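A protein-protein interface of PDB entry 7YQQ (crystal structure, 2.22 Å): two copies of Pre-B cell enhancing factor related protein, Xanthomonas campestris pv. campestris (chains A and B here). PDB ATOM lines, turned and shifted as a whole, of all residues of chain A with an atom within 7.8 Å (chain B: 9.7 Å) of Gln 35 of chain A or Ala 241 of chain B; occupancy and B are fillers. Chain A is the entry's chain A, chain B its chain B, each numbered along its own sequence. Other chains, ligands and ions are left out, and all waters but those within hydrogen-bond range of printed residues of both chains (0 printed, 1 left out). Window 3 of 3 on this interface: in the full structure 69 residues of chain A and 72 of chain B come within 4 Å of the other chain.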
ATOM      1  N   TYR A  28     -17.467  33.774  14.130  1.00  0.00           N
ATOM      2  CA  TYR A  28     -17.322  32.571  14.942  1.00  0.00           C
ATOM      3  C   TYR A  28     -15.926  32.447  15.558  1.00  0.00           C
ATOM      4  O   TYR A  28     -15.774  31.856  16.636  1.00  0.00           O
ATOM      5  CB  TYR A  28     -17.653  31.337  14.108  1.00  0.00           C
ATOM      6  CG  TYR A  28     -16.700  31.065  12.980  1.00  0.00           C
ATOM      7  CD1 TYR A  28     -16.829  31.723  11.765  1.00  0.00           C
ATOM      8  CD2 TYR A  28     -15.693  30.119  13.114  1.00  0.00           C
ATOM      9  CE1 TYR A  28     -15.977  31.459  10.720  1.00  0.00           C
ATOM     10  CE2 TYR A  28     -14.825  29.854  12.074  1.00  0.00           C
ATOM     11  CZ  TYR A  28     -14.971  30.523  10.880  1.00  0.00           C
ATOM     12  OH  TYR A  28     -14.106  30.259   9.840  1.00  0.00           O
ATOM     13  N   LYS A  29     -14.900  32.989  14.903  1.00  0.00           N
ATOM     14  CA  LYS A  29     -13.554  32.866  15.455  1.00  0.00           C
ATOM     15  C   LYS A  29     -13.342  33.740  16.686  1.00  0.00           C
ATOM     16  O   LYS A  29     -12.430  33.462  17.468  1.00  0.00           O
ATOM     17  CB  LYS A  29     -12.504  33.169  14.376  1.00  0.00           C
ATOM     18  CG  LYS A  29     -12.451  32.062  13.314  1.00  0.00           C
ATOM     19  CD  LYS A  29     -11.215  32.119  12.432  1.00  0.00           C
ATOM     20  CE  LYS A  29     -11.589  31.862  10.961  1.00  0.00           C
ATOM     21  NZ  LYS A  29     -11.005  32.857  10.010  1.00  0.00           N
ATOM     22  N   ALA A  30     -14.173  34.766  16.899  1.00  0.00           N
ATOM     23  CA  ALA A  30     -14.081  35.519  18.148  1.00  0.00           C
ATOM     24  C   ALA A  30     -14.350  34.632  19.350  1.00  0.00           C
ATOM     25  O   ALA A  30     -13.838  34.893  20.444  1.00  0.00           O
ATOM     26  CB  ALA A  30     -15.067  36.686  18.152  1.00  0.00           C
ATOM     27  N   SER A  31     -15.162  33.600  19.174  1.00  0.00           N
ATOM     28  CA  SER A  31     -15.546  32.715  20.259  1.00  0.00           C
ATOM     29  C   SER A  31     -14.668  31.466  20.353  1.00  0.00           C
ATOM     30  O   SER A  31     -14.996  30.551  21.111  1.00  0.00           O
ATOM     31  CB  SER A  31     -17.009  32.317  20.091  1.00  0.00           C
ATOM     32  OG  SER A  31     -17.104  31.053  19.451  1.00  0.00           O
ATOM     33  N   HIS A  32     -13.561  31.400  19.606  1.00  0.00           N
ATOM     34  CA  HIS A  32     -12.768  30.173  19.589  1.00  0.00           C
ATOM     35  C   HIS A  32     -12.019  29.908  20.890  1.00  0.00           C
ATOM     36  O   HIS A  32     -11.650  28.758  21.131  1.00  0.00           O
ATOM     37  CB  HIS A  32     -11.765  30.182  18.429  1.00  0.00           C
ATOM     38  CG  HIS A  32     -12.232  29.402  17.243  1.00  0.00           C
ATOM     39  ND1 HIS A  32     -13.419  29.683  16.594  1.00  0.00           N
ATOM     40  CD2 HIS A  32     -11.695  28.339  16.599  1.00  0.00           C
ATOM     41  CE1 HIS A  32     -13.588  28.834  15.595  1.00  0.00           C
ATOM     42  NE2 HIS A  32     -12.553  28.010  15.574  1.00  0.00           N
ATOM     43  N   TRP A  33     -11.755  30.924  21.718  1.00  0.00           N
ATOM     44  CA  TRP A  33     -10.968  30.675  22.927  1.00  0.00           C
ATOM     45  C   TRP A  33     -11.673  29.701  23.862  1.00  0.00           C
ATOM     46  O   TRP A  33     -11.005  29.009  24.631  1.00  0.00           O
ATOM     47  CB  TRP A  33     -10.651  31.991  23.657  1.00  0.00           C
ATOM     48  CG  TRP A  33     -11.616  32.355  24.762  1.00  0.00           C
ATOM     49  CD1 TRP A  33     -11.444  32.165  26.117  1.00  0.00           C
ATOM     50  CD2 TRP A  33     -12.894  32.995  24.610  1.00  0.00           C
ATOM     51  NE1 TRP A  33     -12.535  32.644  26.805  1.00  0.00           N
ATOM     52  CE2 TRP A  33     -13.442  33.158  25.912  1.00  0.00           C
ATOM     53  CE3 TRP A  33     -13.630  33.443  23.505  1.00  0.00           C
ATOM     54  CZ2 TRP A  33     -14.698  33.742  26.132  1.00  0.00           C
ATOM     55  CZ3 TRP A  33     -14.879  34.017  23.728  1.00  0.00           C
ATOM     56  CH2 TRP A  33     -15.400  34.156  25.031  1.00  0.00           C
ATOM     57  N   LEU A  34     -13.007  29.621  23.798  1.00  0.00           N
ATOM     58  CA  LEU A  34     -13.780  28.705  24.628  1.00  0.00           C
ATOM     59  C   LEU A  34     -13.696  27.267  24.154  1.00  0.00           C
ATOM     60  O   LEU A  34     -14.206  26.373  24.835  1.00  0.00           O
ATOM     61  CB  LEU A  34     -15.253  29.110  24.643  1.00  0.00           C
ATOM     62  CG  LEU A  34     -15.660  30.479  25.163  1.00  0.00           C
ATOM     63  CD1 LEU A  34     -17.060  30.811  24.676  1.00  0.00           C
ATOM     64  CD2 LEU A  34     -15.579  30.460  26.682  1.00  0.00           C
ATOM     65  N   GLN A  35     -13.097  27.022  23.001  1.00  0.00           N
ATOM     66  CA  GLN A  35     -13.118  25.702  22.398  1.00  0.00           C
ATOM     67  C   GLN A  35     -11.811  24.957  22.592  1.00  0.00           C
ATOM     68  O   GLN A  35     -11.690  23.812  22.154  1.00  0.00           O
ATOM     69  CB  GLN A  35     -13.469  25.828  20.910  1.00  0.00           C
ATOM     70  CG  GLN A  35     -14.858  26.444  20.695  1.00  0.00           C
ATOM     71  CD  GLN A  35     -15.294  26.425  19.246  1.00  0.00           C
ATOM     72  OE1 GLN A  35     -15.219  25.395  18.577  1.00  0.00           O
ATOM     73  NE2 GLN A  35     -15.753  27.571  18.748  1.00  0.00           N
ATOM     74  N   TYR A  36     -10.849  25.570  23.236  1.00  0.00           N
ATOM     75  CA  TYR A  36      -9.591  24.897  23.476  1.00  0.00           C
ATOM     76  C   TYR A  36      -9.707  23.986  24.700  1.00  0.00           C
ATOM     77  O   TYR A  36     -10.427  24.298  25.648  1.00  0.00           O
ATOM     78  CB  TYR A  36      -8.474  25.920  23.691  1.00  0.00           C
ATOM     79  CG  TYR A  36      -8.005  26.605  22.431  1.00  0.00           C
ATOM     80  CD1 TYR A  36      -7.143  25.962  21.547  1.00  0.00           C
ATOM     81  CD2 TYR A  36      -8.429  27.892  22.116  1.00  0.00           C
ATOM     82  CE1 TYR A  36      -6.710  26.581  20.383  1.00  0.00           C
ATOM     83  CE2 TYR A  36      -7.996  28.528  20.956  1.00  0.00           C
ATOM     84  CZ  TYR A  36      -7.132  27.869  20.098  1.00  0.00           C
ATOM     85  OH  TYR A  36      -6.708  28.491  18.947  1.00  0.00           O
ATOM     86  N   PRO A  37      -9.002  22.863  24.706  1.00  0.00           N
ATOM     87  CA  PRO A  37      -8.936  22.022  25.920  1.00  0.00           C
ATOM     88  C   PRO A  37      -8.547  22.837  27.142  1.00  0.00           C
ATOM     89  O   PRO A  37      -7.924  23.909  27.024  1.00  0.00           O
ATOM     90  CB  PRO A  37      -7.848  20.990  25.576  1.00  0.00           C
ATOM     91  CG  PRO A  37      -7.845  20.922  24.072  1.00  0.00           C
ATOM     92  CD  PRO A  37      -8.237  22.294  23.579  1.00  0.00           C
ATOM     93  N   PRO A  38      -8.916  22.376  28.336  1.00  0.00           N
ATOM     94  CA  PRO A  38      -8.408  23.011  29.557  1.00  0.00           C
ATOM     95  C   PRO A  38      -6.911  22.799  29.681  1.00  0.00           C
ATOM     96  O   PRO A  38      -6.365  21.781  29.246  1.00  0.00           O
ATOM     97  CB  PRO A  38      -9.165  22.289  30.688  1.00  0.00           C
ATOM     98  CG  PRO A  38     -10.309  21.597  30.016  1.00  0.00           C
ATOM     99  CD  PRO A  38      -9.843  21.272  28.628  1.00  0.00           C
ATOM    100  N   THR A  40      -4.729  24.388  28.014  1.00  0.00           N
ATOM    101  CA  THR A  40      -4.003  24.807  26.823  1.00  0.00           C
ATOM    102  C   THR A  40      -3.197  26.069  27.107  1.00  0.00           C
ATOM    103  O   THR A  40      -3.697  27.030  27.704  1.00  0.00           O
ATOM    104  CB  THR A  40      -4.946  25.060  25.650  1.00  0.00           C
ATOM    105  OG1 THR A  40      -5.593  23.836  25.286  1.00  0.00           O
ATOM    106  CG2 THR A  40      -4.152  25.591  24.438  1.00  0.00           C
ATOM    107  N   GLU A  91     -22.547  36.935  19.233  1.00  0.00           N
ATOM    108  CA  GLU A  91     -21.339  36.151  19.421  1.00  0.00           C
ATOM    109  C   GLU A  91     -20.800  36.319  20.832  1.00  0.00           C
ATOM    110  O   GLU A  91     -20.793  37.435  21.356  1.00  0.00           O
ATOM    111  CB  GLU A  91     -20.241  36.569  18.436  1.00  0.00           C
ATOM    112  CG  GLU A  91     -20.398  35.995  17.065  1.00  0.00           C
ATOM    113  CD  GLU A  91     -20.012  34.556  17.024  1.00  0.00           C
ATOM    114  OE1 GLU A  91     -19.199  34.148  17.884  1.00  0.00           O
ATOM    115  OE2 GLU A  91     -20.546  33.835  16.150  1.00  0.00           O
ATOM    116  N   PHE A 139      -2.870  32.706  24.788  1.00  0.00           N
ATOM    117  CA  PHE A 139      -2.398  31.769  23.773  1.00  0.00           C
ATOM    118  C   PHE A 139      -3.282  31.734  22.539  1.00  0.00           C
ATOM    119  O   PHE A 139      -2.860  31.195  21.511  1.00  0.00           O
ATOM    120  CB  PHE A 139      -2.353  30.365  24.359  1.00  0.00           C
ATOM    121  CG  PHE A 139      -3.703  29.872  24.786  1.00  0.00           C
ATOM    122  CD1 PHE A 139      -4.200  30.194  26.037  1.00  0.00           C
ATOM    123  CD2 PHE A 139      -4.489  29.120  23.924  1.00  0.00           C
ATOM    124  CE1 PHE A 139      -5.452  29.764  26.422  1.00  0.00           C
ATOM    125  CE2 PHE A 139      -5.727  28.680  24.299  1.00  0.00           C
ATOM    126  CZ  PHE A 139      -6.220  29.001  25.547  1.00  0.00           C
ATOM    127  N   ILE B 238     -24.707  32.886  14.877  1.00  0.00           N
ATOM    128  CA  ILE B 238     -24.756  32.029  16.061  1.00  0.00           C
ATOM    129  C   ILE B 238     -23.370  31.431  16.276  1.00  0.00           C
ATOM    130  O   ILE B 238     -22.617  31.268  15.306  1.00  0.00           O
ATOM    131  CB  ILE B 238     -25.810  30.923  15.915  1.00  0.00           C
ATOM    132  CG1 ILE B 238     -25.582  30.150  14.611  1.00  0.00           C
ATOM    133  CG2 ILE B 238     -27.214  31.517  15.982  1.00  0.00           C
ATOM    134  CD1 ILE B 238     -26.440  28.909  14.476  1.00  0.00           C
ATOM    135  N   PRO B 239     -22.988  31.110  17.511  1.00  0.00           N
ATOM    136  CA  PRO B 239     -21.708  30.425  17.730  1.00  0.00           C
ATOM    137  C   PRO B 239     -21.730  29.027  17.133  1.00  0.00           C
ATOM    138  O   PRO B 239     -22.776  28.387  17.011  1.00  0.00           O
ATOM    139  CB  PRO B 239     -21.585  30.372  19.259  1.00  0.00           C
ATOM    140  CG  PRO B 239     -22.997  30.469  19.738  1.00  0.00           C
ATOM    141  CD  PRO B 239     -23.722  31.335  18.769  1.00  0.00           C
ATOM    142  N   ALA B 240     -20.547  28.553  16.768  1.00  0.00           N
ATOM    143  CA  ALA B 240     -20.390  27.276  16.084  1.00  0.00           C
ATOM    144  C   ALA B 240     -19.354  26.439  16.827  1.00  0.00           C
ATOM    145  O   ALA B 240     -18.155  26.741  16.774  1.00  0.00           O
ATOM    146  CB  ALA B 240     -19.975  27.492  14.623  1.00  0.00           C
ATOM    147  N   ALA B 241     -19.809  25.391  17.513  1.00  0.00           N
ATOM    148  CA  ALA B 241     -18.895  24.381  18.046  1.00  0.00           C
ATOM    149  C   ALA B 241     -18.229  23.638  16.888  1.00  0.00           C
ATOM    150  O   ALA B 241     -18.856  22.789  16.247  1.00  0.00           O
ATOM    151  CB  ALA B 241     -19.635  23.411  18.961  1.00  0.00           C
ATOM    152  N   GLU B 242     -16.950  23.947  16.632  1.00  0.00           N
ATOM    153  CA  GLU B 242     -16.150  23.318  15.580  1.00  0.00           C
ATOM    154  C   GLU B 242     -15.843  21.846  15.845  1.00  0.00           C
ATOM    155  O   GLU B 242     -15.302  21.182  14.949  1.00  0.00           O
ATOM    156  CB  GLU B 242     -14.840  24.089  15.400  1.00  0.00           C
ATOM    157  CG  GLU B 242     -15.007  25.435  14.743  1.00  0.00           C
ATOM    158  CD  GLU B 242     -15.651  25.300  13.370  1.00  0.00           C
ATOM    159  OE1 GLU B 242     -15.049  24.636  12.499  1.00  0.00           O
ATOM    160  OE2 GLU B 242     -16.773  25.822  13.199  1.00  0.00           O
ATOM    161  N   HIS B 243     -16.226  21.333  17.020  1.00  0.00           N
ATOM    162  CA  HIS B 243     -15.801  20.062  17.605  1.00  0.00           C
ATOM    163  C   HIS B 243     -14.458  19.556  17.090  1.00  0.00           C
ATOM    164  O   HIS B 243     -14.408  18.739  16.161  1.00  0.00           O
ATOM    165  CB  HIS B 243     -16.859  18.958  17.411  1.00  0.00           C
ATOM    166  CG  HIS B 243     -16.623  17.753  18.284  1.00  0.00           C
ATOM    167  ND1 HIS B 243     -15.906  16.655  17.859  1.00  0.00           N
ATOM    168  CD2 HIS B 243     -16.931  17.514  19.583  1.00  0.00           C
ATOM    169  CE1 HIS B 243     -15.826  15.772  18.840  1.00  0.00           C
ATOM    170  NE2 HIS B 243     -16.437  16.268  19.899  1.00  0.00           N
ATOM    171  N   SER B 244     -13.372  20.016  17.709  1.00  0.00           N
ATOM    172  CA  SER B 244     -12.012  19.684  17.294  1.00  0.00           C
ATOM    173  C   SER B 244     -11.726  19.886  15.786  1.00  0.00           C
ATOM    174  O   SER B 244     -11.463  20.998  15.310  1.00  0.00           O
ATOM    175  CB  SER B 244     -11.707  18.239  17.702  1.00  0.00           C
ATOM    176  OG  SER B 244     -10.420  17.822  17.259  1.00  0.00           O
ATOM    177  N   ILE B 271     -29.560  28.781  19.553  1.00  0.00           N
ATOM    178  CA  ILE B 271     -29.245  27.998  18.373  1.00  0.00           C
ATOM    179  C   ILE B 271     -27.742  27.789  18.360  1.00  0.00           C
ATOM    180  O   ILE B 271     -26.984  28.677  18.765  1.00  0.00           O
ATOM    181  CB  ILE B 271     -29.728  28.712  17.089  1.00  0.00           C
ATOM    182  CG1 ILE B 271     -31.175  29.210  17.252  1.00  0.00           C
ATOM    183  CG2 ILE B 271     -29.652  27.790  15.911  1.00  0.00           C
ATOM    184  CD1 ILE B 271     -31.406  30.695  16.913  1.00  0.00           C
ATOM    185  N   VAL B 272     -27.306  26.615  17.913  1.00  0.00           N
ATOM    186  CA  VAL B 272     -25.889  26.273  17.902  1.00  0.00           C
ATOM    187  C   VAL B 272     -25.576  25.506  16.624  1.00  0.00           C
ATOM    188  O   VAL B 272     -26.347  24.635  16.194  1.00  0.00           O
ATOM    189  CB  VAL B 272     -25.495  25.474  19.165  1.00  0.00           C
ATOM    190  CG1 VAL B 272     -26.168  24.082  19.180  1.00  0.00           C
ATOM    191  CG2 VAL B 272     -23.967  25.363  19.280  1.00  0.00           C
ATOM    192  N   ALA B 273     -24.466  25.853  15.989  1.00  0.00           N
ATOM    193  CA  ALA B 273     -23.991  25.104  14.836  1.00  0.00           C
ATOM    194  C   ALA B 273     -22.946  24.091  15.295  1.00  0.00           C
ATOM    195  O   ALA B 273     -22.031  24.443  16.046  1.00  0.00           O
ATOM    196  CB  ALA B 273     -23.401  26.040  13.774  1.00  0.00           C
ATOM    197  N   VAL B 274     -23.084  22.834  14.858  1.00  0.00           N
ATOM    198  CA  VAL B 274     -22.041  21.831  15.042  1.00  0.00           C
ATOM    199  C   VAL B 274     -21.670  21.226  13.689  1.00  0.00           C
ATOM    200  O   VAL B 274     -22.541  20.961  12.852  1.00  0.00           O
ATOM    201  CB  VAL B 274     -22.451  20.736  16.050  1.00  0.00           C
ATOM    202  CG1 VAL B 274     -22.699  21.343  17.425  1.00  0.00           C
ATOM    203  CG2 VAL B 274     -23.662  20.005  15.591  1.00  0.00           C
ATOM    204  N   VAL B 275     -20.372  21.038  13.474  1.00  0.00           N
ATOM    205  CA  VAL B 275     -19.814  20.482  12.245  1.00  0.00           C
ATOM    206  C   VAL B 275     -19.877  18.960  12.301  1.00  0.00           C
ATOM    207  O   VAL B 275     -19.858  18.374  13.384  1.00  0.00           O
ATOM    208  CB  VAL B 275     -18.375  21.000  12.061  1.00  0.00           C
ATOM    209  CG1 VAL B 275     -17.928  20.876  10.609  1.00  0.00           C
ATOM    210  CG2 VAL B 275     -18.320  22.438  12.507  1.00  0.00           C
ATOM    211  N   SER B 276     -19.952  18.307  11.141  1.00  0.00           N
ATOM    212  CA  SER B 276     -20.196  16.863  11.119  1.00  0.00           C
ATOM    213  C   SER B 276     -19.835  16.262   9.757  1.00  0.00           C
ATOM    214  O   SER B 276     -18.977  16.784   9.036  1.00  0.00           O
ATOM    215  CB  SER B 276     -21.660  16.567  11.471  1.00  0.00           C
ATOM    216  OG  SER B 276     -21.795  16.332  12.852  1.00  0.00           O
ATOM    217  N   VAL B 304     -30.145  22.546  17.216  1.00  0.00           N
ATOM    218  CA  VAL B 304     -28.804  22.247  16.741  1.00  0.00           C
ATOM    219  C   VAL B 304     -28.786  22.382  15.228  1.00  0.00           C
ATOM    220  O   VAL B 304     -29.636  21.814  14.534  1.00  0.00           O
ATOM    221  CB  VAL B 304     -28.373  20.834  17.168  1.00  0.00           C
ATOM    222  CG1 VAL B 304     -26.996  20.525  16.609  1.00  0.00           C
ATOM    223  CG2 VAL B 304     -28.394  20.703  18.693  1.00  0.00           C
ATOM    224  N   VAL B 305     -27.818  23.121  14.708  1.00  0.00           N
ATOM    225  CA  VAL B 305     -27.651  23.282  13.275  1.00  0.00           C
ATOM    226  C   VAL B 305     -26.431  22.460  12.876  1.00  0.00           C
ATOM    227  O   VAL B 305     -25.298  22.798  13.230  1.00  0.00           O
ATOM    228  CB  VAL B 305     -27.496  24.763  12.881  1.00  0.00           C
ATOM    229  CG1 VAL B 305     -27.423  24.928  11.365  1.00  0.00           C
ATOM    230  CG2 VAL B 305     -28.633  25.569  13.431  1.00  0.00           C
ATOM    231  N   ILE B 306     -26.649  21.394  12.129  1.00  0.00           N
ATOM    232  CA  ILE B 306     -25.553  20.574  11.632  1.00  0.00           C
ATOM    233  C   ILE B 306     -25.017  21.169  10.333  1.00  0.00           C
ATOM    234  O   ILE B 306     -25.785  21.396   9.386  1.00  0.00           O
ATOM    235  CB  ILE B 306     -26.023  19.134  11.410  1.00  0.00           C
ATOM    236  CG1 ILE B 306     -26.719  18.619  12.666  1.00  0.00           C
ATOM    237  CG2 ILE B 306     -24.857  18.284  10.966  1.00  0.00           C
ATOM    238  CD1 ILE B 306     -25.796  17.937  13.664  1.00  0.00           C
ATOM    239  N   ARG B 307     -23.702  21.421  10.277  1.00  0.00           N
ATOM    240  CA  ARG B 307     -23.055  21.731   9.004  1.00  0.00           C
ATOM    241  C   ARG B 307     -22.185  20.567   8.577  1.00  0.00           C
ATOM    242  O   ARG B 307     -21.096  20.379   9.142  1.00  0.00           O
ATOM    243  CB  ARG B 307     -22.203  22.994   9.068  1.00  0.00           C
ATOM    244  CG  ARG B 307     -21.357  23.120   7.781  1.00  0.00           C
ATOM    245  CD  ARG B 307     -20.829  24.510   7.509  1.00  0.00           C
ATOM    246  NE  ARG B 307     -19.715  24.798   8.398  1.00  0.00           N
ATOM    247  CZ  ARG B 307     -18.440  24.586   8.093  1.00  0.00           C
ATOM    248  NH1 ARG B 307     -18.117  24.093   6.901  1.00  0.00           N
ATOM    249  NH2 ARG B 307     -17.491  24.871   8.980  1.00  0.00           N
ATOM    250  N   ASP B 309     -19.291  19.070   6.465  1.00  0.00           N
ATOM    251  CA  ASP B 309     -18.172  19.715   5.783  1.00  0.00           C
ATOM    252  C   ASP B 309     -17.475  18.761   4.812  1.00  0.00           C
ATOM    253  O   ASP B 309     -16.319  18.988   4.433  1.00  0.00           O
ATOM    254  CB  ASP B 309     -17.187  20.314   6.795  1.00  0.00           C
ATOM    255  CG  ASP B 309     -16.389  19.262   7.540  1.00  0.00           C
ATOM    256  OD1 ASP B 309     -16.815  18.084   7.581  1.00  0.00           O
ATOM    257  OD2 ASP B 309     -15.327  19.621   8.091  1.00  0.00           O
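His 32 of chain A touches just one residue of chain B: Glu 242.
Gln 35 of chain A touches three residues of chain B.
Printed residues of chain B within 4 Å of Glu 91 of chain A: Ile 238 and Pro 239.
Of the printed residues of chain A, Ile 238 of chain B touches Glu 91.
Of the printed residues of chain A, Pro 239 of chain B touches Glu 91 (3.9 Å).
Ala 240 of chain B touches just one residue of chain A: Gln 35 (3.2 Å).
Ala 241 of chain B touches one residue of chain A.
Printed residues of chain A within 4 Å of Glu 242 of chain B: His 32 (3.7 Å) and Gln 35 (3.0 Å).
Val 275 of chain B touches none of the printed residues of chain A.
O of Pro 239 of chain B lies within hydrogen-bond range of N of Ala 273 of chain B (3.2 Å).
A ring nitrogen (ND1) of His 32 of chain A lies within hydrogen-bond range of the backbone carbonyl oxygen of Tyr 28 of chain A, 3.2 Å away.
The backbone NH (N) of Ala 241 of chain B sits at hydrogen-bond distance from the backbone carbonyl oxygen (O) of Ala 273 of chain B (2.8 Å).
Of the 18 printed residues of chain B, 5 touch a printed residue of chain A.
Hydrophobic or aromatic side chains of chain A that line the printed part of chain B: His 32.
Along chain A the printed residues that touch a printed residue of chain B span positions 32 to 91.
Among the printed residues, 6 pairs touch across the chains.
No position is printed for both chains.
Of the 6 pairs that touch across the chains among the printed residues, none has its exchanged pair printed and touching as well.
The side-chain carboxylate (OE2) of Glu 91 of chain A lies close to the backbone carbonyl oxygen (O) of Ile 238 of chain B.
The backbone NH (N) of Glu 242 of chain B lies within hydrogen-bond range of the side-chain amide oxygen (OE1) of Gln 35 of chain A.
The side-chain amide nitrogen of Gln 35 of chain A lies within hydrogen-bond range of the backbone carbonyl oxygen of Ala 240 of chain B, at 3.2 Å.
His 32 of chain A touches Glu 242 of chain B.
Ala 241 of chain B touches Gln 35 of chain A (CA to OE1, 3.9 Å).
OE2 of Glu 91 of chain A touches N of Pro 239 of chain B (3.9 Å).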
